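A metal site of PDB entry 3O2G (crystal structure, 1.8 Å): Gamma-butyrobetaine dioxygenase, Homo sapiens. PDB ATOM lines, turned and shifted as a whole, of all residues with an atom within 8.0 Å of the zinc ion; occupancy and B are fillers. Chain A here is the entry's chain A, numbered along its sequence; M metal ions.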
ATOM      1  N   LEU A  35      -4.180 -15.293   2.629  1.00  0.00           N
ATOM      2  CA  LEU A  35      -4.470 -13.985   2.053  1.00  0.00           C
ATOM      3  C   LEU A  35      -5.569 -13.280   2.875  1.00  0.00           C
ATOM      4  O   LEU A  35      -5.398 -12.131   3.226  1.00  0.00           O
ATOM      5  CB  LEU A  35      -4.890 -14.106   0.581  1.00  0.00           C
ATOM      6  CG  LEU A  35      -3.819 -14.615  -0.392  1.00  0.00           C
ATOM      7  CD1 LEU A  35      -4.504 -15.114  -1.748  1.00  0.00           C
ATOM      8  CD2 LEU A  35      -2.786 -13.521  -0.674  1.00  0.00           C
ATOM      9  N   ARG A  36      -6.672 -13.961   3.170  1.00  0.00           N
ATOM     10  CA  ARG A  36      -7.755 -13.311   3.911  1.00  0.00           C
ATOM     11  C   ARG A  36      -7.271 -12.843   5.297  1.00  0.00           C
ATOM     12  O   ARG A  36      -7.538 -11.703   5.721  1.00  0.00           O
ATOM     13  CB  ARG A  36      -9.008 -14.184   4.034  1.00  0.00           C
ATOM     14  CG  ARG A  36     -10.126 -13.515   4.859  1.00  0.00           C
ATOM     15  CD  ARG A  36     -10.726 -12.329   4.100  1.00  0.00           C
ATOM     16  NE  ARG A  36     -11.708 -11.582   4.907  1.00  0.00           N
ATOM     17  CZ  ARG A  36     -11.389 -10.627   5.770  1.00  0.00           C
ATOM     18  NH1 ARG A  36     -10.118 -10.330   5.992  1.00  0.00           N
ATOM     19  NH2 ARG A  36     -12.321  -9.951   6.422  1.00  0.00           N
ATOM     20  N   ASP A  37      -6.561 -13.744   5.979  1.00  0.00           N
ATOM     21  CA  ASP A  37      -5.994 -13.478   7.309  1.00  0.00           C
ATOM     22  C   ASP A  37      -5.061 -12.276   7.300  1.00  0.00           C
ATOM     23  O   ASP A  37      -4.916 -11.594   8.299  1.00  0.00           O
ATOM     24  CB  ASP A  37      -5.190 -14.719   7.755  1.00  0.00           C
ATOM     25  CG  ASP A  37      -4.522 -14.524   9.127  1.00  0.00           C
ATOM     26  OD1 ASP A  37      -5.275 -14.192  10.054  1.00  0.00           O
ATOM     27  OD2 ASP A  37      -3.275 -14.690   9.244  1.00  0.00           O
ATOM     28  N   ASN A  38      -4.436 -12.024   6.151  1.00  0.00           N
ATOM     29  CA  ASN A  38      -3.459 -10.952   6.006  1.00  0.00           C
ATOM     30  C   ASN A  38      -3.876  -9.773   5.128  1.00  0.00           C
ATOM     31  O   ASN A  38      -3.068  -8.976   4.676  1.00  0.00           O
ATOM     32  CB  ASN A  38      -2.163 -11.597   5.581  1.00  0.00           C
ATOM     33  CG  ASN A  38      -1.569 -12.375   6.716  1.00  0.00           C
ATOM     34  OD1 ASN A  38      -1.302 -11.759   7.758  1.00  0.00           O
ATOM     35  ND2 ASN A  38      -1.390 -13.678   6.570  1.00  0.00           N
ATOM     36  N   CYS A  39      -5.182  -9.629   4.972  1.00  0.00           N
ATOM     37  CA  CYS A  39      -5.739  -8.454   4.295  1.00  0.00           C
ATOM     38  C   CYS A  39      -5.181  -7.188   4.947  1.00  0.00           C
ATOM     39  O   CYS A  39      -5.258  -7.069   6.160  1.00  0.00           O
ATOM     40  CB  CYS A  39      -7.260  -8.438   4.460  1.00  0.00           C
ATOM     41  SG  CYS A  39      -7.996  -6.942   3.677  1.00  0.00           S
ATOM     42  N   PRO A  40      -4.592  -6.281   4.179  1.00  0.00           N
ATOM     43  CA  PRO A  40      -4.017  -5.059   4.758  1.00  0.00           C
ATOM     44  C   PRO A  40      -4.930  -3.856   4.906  1.00  0.00           C
ATOM     45  O   PRO A  40      -4.458  -2.765   5.210  1.00  0.00           O
ATOM     46  CB  PRO A  40      -2.829  -4.753   3.819  1.00  0.00           C
ATOM     47  CG  PRO A  40      -3.243  -5.302   2.512  1.00  0.00           C
ATOM     48  CD  PRO A  40      -4.178  -6.482   2.785  1.00  0.00           C
ATOM     49  N   CYS A  41      -6.235  -4.022   4.678  1.00  0.00           N
ATOM     50  CA  CYS A  41      -7.149  -2.901   4.746  1.00  0.00           C
ATOM     51  C   CYS A  41      -7.291  -2.436   6.210  1.00  0.00           C
ATOM     52  O   CYS A  41      -6.925  -3.162   7.149  1.00  0.00           O
ATOM     53  CB  CYS A  41      -8.526  -3.247   4.152  1.00  0.00           C
ATOM     54  SG  CYS A  41      -9.712  -4.033   5.324  1.00  0.00           S
ATOM     55  N   SER A  42      -7.883  -1.268   6.383  1.00  0.00           N
ATOM     56  CA  SER A  42      -7.941  -0.625   7.690  1.00  0.00           C
ATOM     57  C   SER A  42      -8.872  -1.363   8.655  1.00  0.00           C
ATOM     58  O   SER A  42      -8.696  -1.233   9.872  1.00  0.00           O
ATOM     59  CB  SER A  42      -8.328   0.826   7.598  1.00  0.00           C
ATOM     60  OG  SER A  42      -9.628   0.968   7.083  1.00  0.00           O
ATOM     61  N   ASP A  43      -9.810  -2.158   8.144  1.00  0.00           N
ATOM     62  CA  ASP A  43     -10.633  -2.991   9.051  1.00  0.00           C
ATOM     63  C   ASP A  43      -9.822  -4.133   9.657  1.00  0.00           C
ATOM     64  O   ASP A  43     -10.044  -4.492  10.818  1.00  0.00           O
ATOM     65  CB  ASP A  43     -11.848  -3.623   8.390  1.00  0.00           C
ATOM     66  CG  ASP A  43     -12.826  -2.615   7.795  1.00  0.00           C
ATOM     67  OD1 ASP A  43     -12.803  -1.414   8.109  1.00  0.00           O
ATOM     68  OD2 ASP A  43     -13.701  -3.087   7.078  1.00  0.00           O
ATOM     69  N   CYS A  44      -8.863  -4.652   8.891  1.00  0.00           N
ATOM     70  CA  CYS A  44      -8.188  -5.886   9.219  1.00  0.00           C
ATOM     71  C   CYS A  44      -6.840  -5.667   9.818  1.00  0.00           C
ATOM     72  O   CYS A  44      -6.287  -6.560  10.417  1.00  0.00           O
ATOM     73  CB  CYS A  44      -8.006  -6.741   7.949  1.00  0.00           C
ATOM     74  SG  CYS A  44      -9.565  -7.314   7.244  1.00  0.00           S
ATOM     75  N   TYR A  45      -6.275  -4.470   9.627  1.00  0.00           N
ATOM     76  CA  TYR A  45      -4.864  -4.212   9.892  1.00  0.00           C
ATOM     77  C   TYR A  45      -4.645  -2.812  10.365  1.00  0.00           C
ATOM     78  O   TYR A  45      -5.125  -1.846   9.747  1.00  0.00           O
ATOM     79  CB  TYR A  45      -4.063  -4.466   8.590  1.00  0.00           C
ATOM     80  CG  TYR A  45      -2.578  -4.526   8.776  1.00  0.00           C
ATOM     81  CD1 TYR A  45      -1.982  -5.723   9.165  1.00  0.00           C
ATOM     82  CD2 TYR A  45      -1.769  -3.409   8.582  1.00  0.00           C
ATOM     83  CE1 TYR A  45      -0.614  -5.819   9.324  1.00  0.00           C
ATOM     84  CE2 TYR A  45      -0.383  -3.497   8.764  1.00  0.00           C
ATOM     85  CZ  TYR A  45       0.167  -4.696   9.124  1.00  0.00           C
ATOM     86  OH  TYR A  45       1.497  -4.860   9.339  1.00  0.00           O
ATOM     87  N   LEU A  54      -7.728  -8.163  12.591  1.00  0.00           N
ATOM     88  CA  LEU A  54      -8.638  -9.263  12.269  1.00  0.00           C
ATOM     89  C   LEU A  54      -8.530 -10.343  13.361  1.00  0.00           C
ATOM     90  O   LEU A  54      -7.433 -10.707  13.771  1.00  0.00           O
ATOM     91  CB  LEU A  54      -8.308  -9.877  10.895  1.00  0.00           C
ATOM     92  CG  LEU A  54      -9.298 -10.884  10.316  1.00  0.00           C
ATOM     93  CD1 LEU A  54     -10.575 -10.203   9.852  1.00  0.00           C
ATOM     94  CD2 LEU A  54      -8.602 -11.700   9.127  1.00  0.00           C
ATOM     95  N   TRP A  79     -14.036 -11.387  -1.735  1.00  0.00           N
ATOM     96  CA  TRP A  79     -14.314 -12.550  -0.919  1.00  0.00           C
ATOM     97  C   TRP A  79     -15.816 -12.898  -0.908  1.00  0.00           C
ATOM     98  O   TRP A  79     -16.641 -12.051  -1.221  1.00  0.00           O
ATOM     99  CB  TRP A  79     -13.789 -12.335   0.505  1.00  0.00           C
ATOM    100  CG  TRP A  79     -12.287 -12.085   0.541  1.00  0.00           C
ATOM    101  CD1 TRP A  79     -11.647 -10.912   0.832  1.00  0.00           C
ATOM    102  CD2 TRP A  79     -11.285 -13.065   0.353  1.00  0.00           C
ATOM    103  NE1 TRP A  79     -10.275 -11.107   0.782  1.00  0.00           N
ATOM    104  CE2 TRP A  79     -10.037 -12.430   0.495  1.00  0.00           C
ATOM    105  CE3 TRP A  79     -11.316 -14.411   0.030  1.00  0.00           C
ATOM    106  CZ2 TRP A  79      -8.835 -13.111   0.358  1.00  0.00           C
ATOM    107  CZ3 TRP A  79     -10.106 -15.104  -0.104  1.00  0.00           C
ATOM    108  CH2 TRP A  79      -8.896 -14.438   0.047  1.00  0.00           C
ATOM    109  N   HIS A  83     -16.179  -8.910   1.447  1.00  0.00           N
ATOM    110  CA  HIS A  83     -14.989  -8.220   1.858  1.00  0.00           C
ATOM    111  C   HIS A  83     -14.078  -8.076   0.635  1.00  0.00           C
ATOM    112  O   HIS A  83     -14.158  -8.880  -0.300  1.00  0.00           O
ATOM    113  CB  HIS A  83     -14.260  -8.971   2.972  1.00  0.00           C
ATOM    114  CG  HIS A  83     -13.293  -8.106   3.704  1.00  0.00           C
ATOM    115  ND1 HIS A  83     -13.716  -7.152   4.603  1.00  0.00           N
ATOM    116  CD2 HIS A  83     -11.938  -8.007   3.644  1.00  0.00           C
ATOM    117  CE1 HIS A  83     -12.648  -6.517   5.082  1.00  0.00           C
ATOM    118  NE2 HIS A  83     -11.562  -6.995   4.488  1.00  0.00           N
ATOM    119  N   TYR A  84     -13.252  -7.041   0.664  1.00  0.00           N
ATOM    120  CA  TYR A  84     -12.426  -6.694  -0.494  1.00  0.00           C
ATOM    121  C   TYR A  84     -11.008  -6.429  -0.065  1.00  0.00           C
ATOM    122  O   TYR A  84     -10.796  -5.750   0.957  1.00  0.00           O
ATOM    123  CB  TYR A  84     -13.008  -5.463  -1.195  1.00  0.00           C
ATOM    124  CG  TYR A  84     -12.079  -4.869  -2.240  1.00  0.00           C
ATOM    125  CD1 TYR A  84     -11.853  -5.510  -3.454  1.00  0.00           C
ATOM    126  CD2 TYR A  84     -11.420  -3.678  -2.021  1.00  0.00           C
ATOM    127  CE1 TYR A  84     -11.015  -4.997  -4.410  1.00  0.00           C
ATOM    128  CE2 TYR A  84     -10.530  -3.137  -2.992  1.00  0.00           C
ATOM    129  CZ  TYR A  84     -10.378  -3.782  -4.209  1.00  0.00           C
ATOM    130  OH  TYR A  84      -9.526  -3.263  -5.174  1.00  0.00           O
ATOM    131  N   SER A  85     -10.044  -7.015  -0.777  1.00  0.00           N
ATOM    132  CA  SER A  85      -8.630  -6.910  -0.394  1.00  0.00           C
ATOM    133  C   SER A  85      -7.705  -6.557  -1.566  1.00  0.00           C
ATOM    134  O   SER A  85      -7.920  -7.020  -2.695  1.00  0.00           O
ATOM    135  CB  SER A  85      -8.089  -8.200   0.247  1.00  0.00           C
ATOM    136  OG  SER A  85      -8.911  -8.738   1.292  1.00  0.00           O
ATOM    137  N   GLU A  86      -6.642  -5.797  -1.273  1.00  0.00           N
ATOM    138  CA  GLU A  86      -5.589  -5.509  -2.286  1.00  0.00           C
ATOM    139  C   GLU A  86      -4.255  -5.958  -1.756  1.00  0.00           C
ATOM    140  O   GLU A  86      -3.940  -5.670  -0.589  1.00  0.00           O
ATOM    141  CB  GLU A  86      -5.531  -4.004  -2.581  1.00  0.00           C
ATOM    142  CG  GLU A  86      -6.785  -3.460  -3.194  1.00  0.00           C
ATOM    143  CD  GLU A  86      -6.689  -2.045  -3.653  1.00  0.00           C
ATOM    144  OE1 GLU A  86      -5.656  -1.389  -3.421  1.00  0.00           O
ATOM    145  OE2 GLU A  86      -7.690  -1.571  -4.248  1.00  0.00           O
ATOM    146  N   PHE A  87      -3.471  -6.698  -2.560  1.00  0.00           N
ATOM    147  CA  PHE A  87      -2.120  -7.144  -2.151  1.00  0.00           C
ATOM    148  C   PHE A  87      -1.101  -6.682  -3.167  1.00  0.00           C
ATOM    149  O   PHE A  87      -1.315  -6.775  -4.409  1.00  0.00           O
ATOM    150  CB  PHE A  87      -2.029  -8.651  -2.002  1.00  0.00           C
ATOM    151  CG  PHE A  87      -3.073  -9.232  -1.084  1.00  0.00           C
ATOM    152  CD1 PHE A  87      -2.828  -9.321   0.264  1.00  0.00           C
ATOM    153  CD2 PHE A  87      -4.300  -9.643  -1.568  1.00  0.00           C
ATOM    154  CE1 PHE A  87      -3.815  -9.840   1.132  1.00  0.00           C
ATOM    155  CE2 PHE A  87      -5.254 -10.195  -0.740  1.00  0.00           C
ATOM    156  CZ  PHE A  87      -5.013 -10.280   0.627  1.00  0.00           C
HETATM  157 ZN    ZN M   1      -9.642  -6.320   5.131  1.00  0.00          ZN
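The zinc ion is bound by NE2 of His 83 (2.1 Å). SG of Cys 39 is bound to the zinc ion (2.3 Å). The zinc ion is bound by SG of Cys 41. The side-chain sulfur (SG) of Cys 44 binds the zinc ion, 2.3 Å away.
Within 4 Å of the zinc ion: Cys 39, Cys 41, Cys 44 and His 83. The nearest printed residue that does not touch the zinc ion is Arg 36 (4.1 Å).
N of Leu 54 is in hydrogen-bond range of O of Cys 44, 3.1 Å away. SG of Cys 41 lies close to N of Asp 43, 3.4 Å away. The side-chain sulfur (SG) of Cys 44 lies close to the guanidinium group (NH1) of Arg 36, 3.3 Å away. The side-chain sulfur (SG) of Cys 39 sits close to the side-chain hydroxyl (OG) of Ser 85, at 3.1 Å.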
